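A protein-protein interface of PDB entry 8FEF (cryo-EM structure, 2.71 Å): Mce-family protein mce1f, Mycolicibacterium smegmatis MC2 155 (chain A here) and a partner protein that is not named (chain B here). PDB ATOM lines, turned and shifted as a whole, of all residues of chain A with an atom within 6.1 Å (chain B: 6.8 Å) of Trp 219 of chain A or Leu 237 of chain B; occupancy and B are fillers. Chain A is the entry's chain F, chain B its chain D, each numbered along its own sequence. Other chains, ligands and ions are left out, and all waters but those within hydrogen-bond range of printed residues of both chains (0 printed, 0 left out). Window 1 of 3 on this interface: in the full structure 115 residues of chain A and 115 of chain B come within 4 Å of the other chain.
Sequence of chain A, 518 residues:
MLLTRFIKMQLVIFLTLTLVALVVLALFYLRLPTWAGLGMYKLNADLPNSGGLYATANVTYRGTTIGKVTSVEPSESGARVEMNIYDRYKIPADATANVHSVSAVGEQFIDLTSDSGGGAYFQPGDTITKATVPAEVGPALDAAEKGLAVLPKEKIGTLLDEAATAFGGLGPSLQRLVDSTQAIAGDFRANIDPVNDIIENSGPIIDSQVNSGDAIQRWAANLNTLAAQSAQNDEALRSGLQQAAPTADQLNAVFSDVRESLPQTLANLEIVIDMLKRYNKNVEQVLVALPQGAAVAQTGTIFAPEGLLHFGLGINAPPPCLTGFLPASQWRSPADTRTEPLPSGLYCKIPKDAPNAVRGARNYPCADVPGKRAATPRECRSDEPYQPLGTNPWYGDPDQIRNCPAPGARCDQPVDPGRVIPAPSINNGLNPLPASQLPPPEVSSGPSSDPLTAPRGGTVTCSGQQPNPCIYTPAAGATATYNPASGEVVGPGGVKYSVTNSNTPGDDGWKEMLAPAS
N of Asn 242 of chain B sits close to ND2 of Asn 222 of chain A.
The side-chain hydroxyl of Thr 241 of chain B sits close to the side-chain amide nitrogen of Asn 222 of chain A, 3.3 Å away.
The side-chain amide oxygen of Asn 242 of chain B sits at hydrogen-bond distance from the guanidinium group of Arg 218 of chain A (3.0 Å).
O of Ala 238 of chain B lies within hydrogen-bond range of OG1 of Thr 241 of chain B (2.9 Å).
OD1 of Asn 222 of chain A lies close to NE of Arg 218 of chain A, at 3.3 Å.
The backbone carbonyl oxygen (O) of Ala 238 of chain B sits close to the side-chain amide oxygen (OD1) of Asn 242 of chain B.
The backbone carbonyl oxygen of Leu 237 of chain B is in hydrogen-bond range of the side-chain hydroxyl of Thr 241 of chain B (3.0 Å).
Among the printed residues, pairs that only touch across the chains: Ala 215 of chain A with Asn 234 of chain B (3.6 Å), Ala 215 of chain A with Asn 235 of chain B (3.4 Å), Ala 215 of chain A with Ala 238 of chain B (3.5 Å), Ile 216 of chain A with Asn 234 of chain B (3.4 Å), Trp 219 of chain A with Asn 234 of chain B (3.9 Å), Trp 219 of chain A with Leu 237 of chain B (3.5 Å), Trp 219 of chain A with Ala 238 of chain B (3.8 Å) and Trp 219 of chain A with Thr 241 of chain B (3.6 Å).
Of the printed residues of chain A, Leu 237 of chain B touches Trp 219.
Of the printed residues of chain A, Asn 235 of chain B touches Ala 215.
Of the printed residues of chain A, Asn 242 of chain B touches Arg 218 (3.0 Å) and Asn 222 (2.3 Å).
Printed residues of chain B within 4 Å of Ala 215 of chain A: Asn 234, Asn 235 and Ala 238.
Printed residues of chain A within 4 Å of Asn 234 of chain B: Ala 215, Ile 216 and Trp 219.
Printed residues of chain A within 4 Å of Ala 238 of chain B: Ala 215 (3.5 Å) and Trp 219 (3.8 Å).
The nearest residue of chain B that does not touch Trp 219 of chain A is Asn 242 of chain B (5.7 Å).
The nearest residue of chain A that does not touch Leu 237 of chain B is Ala 215 of chain A (5.8 Å).
Printed residues of chain A that touch a printed residue of chain B: Ala 215, Ile 216, Arg 218, Trp 219 and Asn 222.
Along chain A the printed residues that touch a printed residue of chain B span positions 215 to 222.
Among the printed residues, 11 pairs touch across the chains.
Among the printed residues, no Asp or Glu carboxylate lies within 4 Å of a Lys or Arg side-chain nitrogen of the other chain.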
ATOM      1  N   ASP A 214     -12.514  24.463   9.884  1.00  0.00           N
ATOM      2  CA  ASP A 214     -12.629  25.906  10.068  1.00  0.00           C
ATOM      3  C   ASP A 214     -14.085  26.348  10.012  1.00  0.00           C
ATOM      4  O   ASP A 214     -14.517  27.192  10.806  1.00  0.00           O
ATOM      5  CB  ASP A 214     -11.804  26.635   9.009  1.00  0.00           C
ATOM      6  CG  ASP A 214     -10.335  26.715   9.368  1.00  0.00           C
ATOM      7  OD1 ASP A 214     -10.020  26.836  10.570  1.00  0.00           O
ATOM      8  OD2 ASP A 214      -9.494  26.657   8.447  1.00  0.00           O
ATOM      9  N   ALA A 215     -14.857  25.776   9.086  1.00  0.00           N
ATOM     10  CA  ALA A 215     -16.269  26.126   8.971  1.00  0.00           C
ATOM     11  C   ALA A 215     -17.048  25.723  10.218  1.00  0.00           C
ATOM     12  O   ALA A 215     -17.911  26.476  10.686  1.00  0.00           O
ATOM     13  CB  ALA A 215     -16.873  25.472   7.729  1.00  0.00           C
ATOM     14  N   ILE A 216     -16.772  24.535  10.766  1.00  0.00           N
ATOM     15  CA  ILE A 216     -17.524  24.106  11.942  1.00  0.00           C
ATOM     16  C   ILE A 216     -17.135  24.934  13.159  1.00  0.00           C
ATOM     17  O   ILE A 216     -17.989  25.271  13.985  1.00  0.00           O
ATOM     18  CB  ILE A 216     -17.398  22.588  12.187  1.00  0.00           C
ATOM     19  CG1 ILE A 216     -16.058  22.191  12.797  1.00  0.00           C
ATOM     20  CG2 ILE A 216     -17.642  21.817  10.906  1.00  0.00           C
ATOM     21  CD1 ILE A 216     -16.035  20.753  13.225  1.00  0.00           C
ATOM     22  N   GLN A 217     -15.855  25.302  13.280  1.00  0.00           N
ATOM     23  CA  GLN A 217     -15.464  26.203  14.360  1.00  0.00           C
ATOM     24  C   GLN A 217     -16.155  27.554  14.219  1.00  0.00           C
ATOM     25  O   GLN A 217     -16.623  28.130  15.211  1.00  0.00           O
ATOM     26  CB  GLN A 217     -13.946  26.373  14.383  1.00  0.00           C
ATOM     27  CG  GLN A 217     -13.190  25.110  14.741  1.00  0.00           C
ATOM     28  CD  GLN A 217     -11.693  25.316  14.761  1.00  0.00           C
ATOM     29  OE1 GLN A 217     -11.208  26.438  14.629  1.00  0.00           O
ATOM     30  NE2 GLN A 217     -10.949  24.229  14.926  1.00  0.00           N
ATOM     31  N   ARG A 218     -16.244  28.066  12.989  1.00  0.00           N
ATOM     32  CA  ARG A 218     -16.871  29.363  12.768  1.00  0.00           C
ATOM     33  C   ARG A 218     -18.356  29.329  13.109  1.00  0.00           C
ATOM     34  O   ARG A 218     -18.864  30.237  13.779  1.00  0.00           O
ATOM     35  CB  ARG A 218     -16.661  29.814  11.324  1.00  0.00           C
ATOM     36  CG  ARG A 218     -17.207  31.199  11.033  1.00  0.00           C
ATOM     37  CD  ARG A 218     -16.680  32.214  12.032  1.00  0.00           C
ATOM     38  NE  ARG A 218     -17.277  33.530  11.844  1.00  0.00           N
ATOM     39  CZ  ARG A 218     -17.083  34.562  12.653  1.00  0.00           C
ATOM     40  NH1 ARG A 218     -16.318  34.462  13.727  1.00  0.00           N
ATOM     41  NH2 ARG A 218     -17.675  35.721  12.381  1.00  0.00           N
ATOM     42  N   TRP A 219     -19.076  28.295  12.663  1.00  0.00           N
ATOM     43  CA  TRP A 219     -20.498  28.284  12.992  1.00  0.00           C
ATOM     44  C   TRP A 219     -20.743  27.919  14.447  1.00  0.00           C
ATOM     45  O   TRP A 219     -21.773  28.315  14.992  1.00  0.00           O
ATOM     46  CB  TRP A 219     -21.321  27.383  12.050  1.00  0.00           C
ATOM     47  CG  TRP A 219     -21.171  25.877  12.123  1.00  0.00           C
ATOM     48  CD1 TRP A 219     -20.624  25.079  11.165  1.00  0.00           C
ATOM     49  CD2 TRP A 219     -21.647  24.989  13.154  1.00  0.00           C
ATOM     50  NE1 TRP A 219     -20.690  23.762  11.544  1.00  0.00           N
ATOM     51  CE2 TRP A 219     -21.309  23.680  12.761  1.00  0.00           C
ATOM     52  CE3 TRP A 219     -22.308  25.174  14.372  1.00  0.00           C
ATOM     53  CZ2 TRP A 219     -21.606  22.566  13.543  1.00  0.00           C
ATOM     54  CZ3 TRP A 219     -22.595  24.068  15.147  1.00  0.00           C
ATOM     55  CH2 TRP A 219     -22.247  22.781  14.729  1.00  0.00           C
ATOM     56  N   ALA A 220     -19.817  27.218  15.108  1.00  0.00           N
ATOM     57  CA  ALA A 220     -19.941  27.030  16.549  1.00  0.00           C
ATOM     58  C   ALA A 220     -19.814  28.357  17.286  1.00  0.00           C
ATOM     59  O   ALA A 220     -20.610  28.661  18.184  1.00  0.00           O
ATOM     60  CB  ALA A 220     -18.890  26.035  17.040  1.00  0.00           C
ATOM     61  N   ALA A 221     -18.826  29.172  16.904  1.00  0.00           N
ATOM     62  CA  ALA A 221     -18.672  30.486  17.524  1.00  0.00           C
ATOM     63  C   ALA A 221     -19.876  31.380  17.242  1.00  0.00           C
ATOM     64  O   ALA A 221     -20.350  32.100  18.132  1.00  0.00           O
ATOM     65  CB  ALA A 221     -17.385  31.147  17.035  1.00  0.00           C
ATOM     66  N   ASN A 222     -20.387  31.346  16.011  1.00  0.00           N
ATOM     67  CA  ASN A 222     -21.539  32.174  15.669  1.00  0.00           C
ATOM     68  C   ASN A 222     -22.805  31.693  16.369  1.00  0.00           C
ATOM     69  O   ASN A 222     -23.656  32.507  16.743  1.00  0.00           O
ATOM     70  CB  ASN A 222     -21.735  32.201  14.160  1.00  0.00           C
ATOM     71  CG  ASN A 222     -20.657  32.983  13.451  1.00  0.00           C
ATOM     72  OD1 ASN A 222     -19.691  33.430  14.067  1.00  0.00           O
ATOM     73  ND2 ASN A 222     -20.816  33.153  12.148  1.00  0.00           N
ATOM     74  N   LEU A 223     -22.957  30.378  16.537  1.00  0.00           N
ATOM     75  CA  LEU A 223     -24.067  29.852  17.321  1.00  0.00           C
ATOM     76  C   LEU A 223     -23.976  30.324  18.761  1.00  0.00           C
ATOM     77  O   LEU A 223     -24.984  30.715  19.356  1.00  0.00           O
ATOM     78  CB  LEU A 223     -24.080  28.326  17.258  1.00  0.00           C
ATOM     79  CG  LEU A 223     -25.080  27.615  18.172  1.00  0.00           C
ATOM     80  CD1 LEU A 223     -26.504  27.842  17.693  1.00  0.00           C
ATOM     81  CD2 LEU A 223     -24.767  26.132  18.261  1.00  0.00           C
ATOM     82  N   ASN A 224     -22.769  30.299  19.332  1.00  0.00           N
ATOM     83  CA  ASN A 224     -22.572  30.820  20.680  1.00  0.00           C
ATOM     84  C   ASN A 224     -23.006  32.278  20.768  1.00  0.00           C
ATOM     85  O   ASN A 224     -23.753  32.662  21.675  1.00  0.00           O
ATOM     86  CB  ASN A 224     -21.105  30.665  21.084  1.00  0.00           C
ATOM     87  CG  ASN A 224     -20.824  31.178  22.483  1.00  0.00           C
ATOM     88  OD1 ASN A 224     -21.727  31.300  23.308  1.00  0.00           O
ATOM     89  ND2 ASN A 224     -19.560  31.476  22.755  1.00  0.00           N
ATOM     90  N   ALA B 232     -19.957  20.835   1.979  1.00  0.00           N
ATOM     91  CA  ALA B 232     -20.779  21.956   1.543  1.00  0.00           C
ATOM     92  C   ALA B 232     -21.752  22.382   2.633  1.00  0.00           C
ATOM     93  O   ALA B 232     -22.019  23.573   2.801  1.00  0.00           O
ATOM     94  CB  ALA B 232     -21.527  21.590   0.263  1.00  0.00           C
ATOM     95  N   LEU B 233     -22.301  21.418   3.378  1.00  0.00           N
ATOM     96  CA  LEU B 233     -23.212  21.741   4.472  1.00  0.00           C
ATOM     97  C   LEU B 233     -22.508  22.537   5.557  1.00  0.00           C
ATOM     98  O   LEU B 233     -23.058  23.517   6.070  1.00  0.00           O
ATOM     99  CB  LEU B 233     -23.806  20.460   5.053  1.00  0.00           C
ATOM    100  CG  LEU B 233     -24.562  20.586   6.376  1.00  0.00           C
ATOM    101  CD1 LEU B 233     -25.789  21.468   6.229  1.00  0.00           C
ATOM    102  CD2 LEU B 233     -24.944  19.216   6.895  1.00  0.00           C
ATOM    103  N   ASN B 234     -21.293  22.128   5.924  1.00  0.00           N
ATOM    104  CA  ASN B 234     -20.543  22.872   6.931  1.00  0.00           C
ATOM    105  C   ASN B 234     -20.248  24.291   6.460  1.00  0.00           C
ATOM    106  O   ASN B 234     -20.426  25.255   7.218  1.00  0.00           O
ATOM    107  CB  ASN B 234     -19.250  22.136   7.274  1.00  0.00           C
ATOM    108  CG  ASN B 234     -19.487  20.921   8.144  1.00  0.00           C
ATOM    109  OD1 ASN B 234     -20.397  20.905   8.968  1.00  0.00           O
ATOM    110  ND2 ASN B 234     -18.660  19.898   7.972  1.00  0.00           N
ATOM    111  N   ASN B 235     -19.813  24.442   5.205  1.00  0.00           N
ATOM    112  CA  ASN B 235     -19.511  25.776   4.691  1.00  0.00           C
ATOM    113  C   ASN B 235     -20.764  26.646   4.612  1.00  0.00           C
ATOM    114  O   ASN B 235     -20.726  27.833   4.963  1.00  0.00           O
ATOM    115  CB  ASN B 235     -18.837  25.671   3.325  1.00  0.00           C
ATOM    116  CG  ASN B 235     -17.436  25.105   3.413  1.00  0.00           C
ATOM    117  OD1 ASN B 235     -16.695  25.396   4.350  1.00  0.00           O
ATOM    118  ND2 ASN B 235     -17.065  24.290   2.435  1.00  0.00           N
ATOM    119  N   ASP B 236     -21.882  26.076   4.158  1.00  0.00           N
ATOM    120  CA  ASP B 236     -23.126  26.833   4.064  1.00  0.00           C
ATOM    121  C   ASP B 236     -23.637  27.226   5.441  1.00  0.00           C
ATOM    122  O   ASP B 236     -24.167  28.326   5.617  1.00  0.00           O
ATOM    123  CB  ASP B 236     -24.182  26.025   3.311  1.00  0.00           C
ATOM    124  CG  ASP B 236     -23.823  25.808   1.858  1.00  0.00           C
ATOM    125  OD1 ASP B 236     -22.718  26.220   1.448  1.00  0.00           O
ATOM    126  OD2 ASP B 236     -24.644  25.218   1.126  1.00  0.00           O
ATOM    127  N   LEU B 237     -23.507  26.332   6.424  1.00  0.00           N
ATOM    128  CA  LEU B 237     -23.905  26.660   7.787  1.00  0.00           C
ATOM    129  C   LEU B 237     -23.060  27.797   8.341  1.00  0.00           C
ATOM    130  O   LEU B 237     -23.587  28.718   8.977  1.00  0.00           O
ATOM    131  CB  LEU B 237     -23.794  25.417   8.668  1.00  0.00           C
ATOM    132  CG  LEU B 237     -24.358  25.492  10.083  1.00  0.00           C
ATOM    133  CD1 LEU B 237     -25.820  25.890  10.047  1.00  0.00           C
ATOM    134  CD2 LEU B 237     -24.184  24.154  10.772  1.00  0.00           C
ATOM    135  N   ALA B 238     -21.746  27.751   8.100  1.00  0.00           N
ATOM    136  CA  ALA B 238     -20.876  28.833   8.548  1.00  0.00           C
ATOM    137  C   ALA B 238     -21.265  30.157   7.900  1.00  0.00           C
ATOM    138  O   ALA B 238     -21.333  31.187   8.577  1.00  0.00           O
ATOM    139  CB  ALA B 238     -19.417  28.496   8.245  1.00  0.00           C
ATOM    140  N   GLN B 239     -21.533  30.147   6.592  1.00  0.00           N
ATOM    141  CA  GLN B 239     -21.920  31.379   5.905  1.00  0.00           C
ATOM    142  C   GLN B 239     -23.265  31.902   6.404  1.00  0.00           C
ATOM    143  O   GLN B 239     -23.436  33.112   6.603  1.00  0.00           O
ATOM    144  CB  GLN B 239     -21.959  31.139   4.397  1.00  0.00           C
ATOM    145  CG  GLN B 239     -22.333  32.357   3.573  1.00  0.00           C
ATOM    146  CD  GLN B 239     -22.477  32.034   2.098  1.00  0.00           C
ATOM    147  OE1 GLN B 239     -22.279  30.893   1.679  1.00  0.00           O
ATOM    148  NE2 GLN B 239     -22.824  33.037   1.303  1.00  0.00           N
ATOM    149  N   PHE B 240     -24.232  31.004   6.609  1.00  0.00           N
ATOM    150  CA  PHE B 240     -25.555  31.411   7.069  1.00  0.00           C
ATOM    151  C   PHE B 240     -25.495  32.011   8.467  1.00  0.00           C
ATOM    152  O   PHE B 240     -26.178  32.999   8.756  1.00  0.00           O
ATOM    153  CB  PHE B 240     -26.502  30.213   7.031  1.00  0.00           C
ATOM    154  CG  PHE B 240     -27.893  30.521   7.499  1.00  0.00           C
ATOM    155  CD1 PHE B 240     -28.743  31.294   6.729  1.00  0.00           C
ATOM    156  CD2 PHE B 240     -28.356  30.022   8.705  1.00  0.00           C
ATOM    157  CE1 PHE B 240     -30.024  31.572   7.158  1.00  0.00           C
ATOM    158  CE2 PHE B 240     -29.637  30.298   9.137  1.00  0.00           C
ATOM    159  CZ  PHE B 240     -30.472  31.073   8.362  1.00  0.00           C
ATOM    160  N   THR B 241     -24.691  31.421   9.354  1.00  0.00           N
ATOM    161  CA  THR B 241     -24.518  32.007  10.678  1.00  0.00           C
ATOM    162  C   THR B 241     -23.717  33.305  10.628  1.00  0.00           C
ATOM    163  O   THR B 241     -23.950  34.201  11.447  1.00  0.00           O
ATOM    164  CB  THR B 241     -23.857  31.001  11.617  1.00  0.00           C
ATOM    165  OG1 THR B 241     -22.611  30.568  11.061  1.00  0.00           O
ATOM    166  CG2 THR B 241     -24.763  29.804  11.837  1.00  0.00           C
ATOM    167  N   ASN B 242     -22.774  33.427   9.687  1.00  0.00           N
ATOM    168  CA  ASN B 242     -22.091  34.701   9.478  1.00  0.00           C
ATOM    169  C   ASN B 242     -23.052  35.788   9.019  1.00  0.00           C
ATOM    170  O   ASN B 242     -22.821  36.972   9.286  1.00  0.00           O
ATOM    171  CB  ASN B 242     -20.969  34.541   8.451  1.00  0.00           C
ATOM    172  CG  ASN B 242     -19.754  33.840   9.015  1.00  0.00           C
ATOM    173  OD1 ASN B 242     -19.769  33.356  10.143  1.00  0.00           O
ATOM    174  ND2 ASN B 242     -18.689  33.780   8.225  1.00  0.00           N
ATOM    175  N   SER B 243     -24.118  35.409   8.310  1.00  0.00           N
ATOM    176  CA  SER B 243     -25.075  36.395   7.816  1.00  0.00           C
ATOM    177  C   SER B 243     -25.759  37.173   8.936  1.00  0.00           C
ATOM    178  O   SER B 243     -26.293  38.258   8.681  1.00  0.00           O
ATOM    179  CB  SER B 243     -26.133  35.716   6.946  1.00  0.00           C
ATOM    180  OG  SER B 243     -25.548  35.100   5.815  1.00  0.00           O
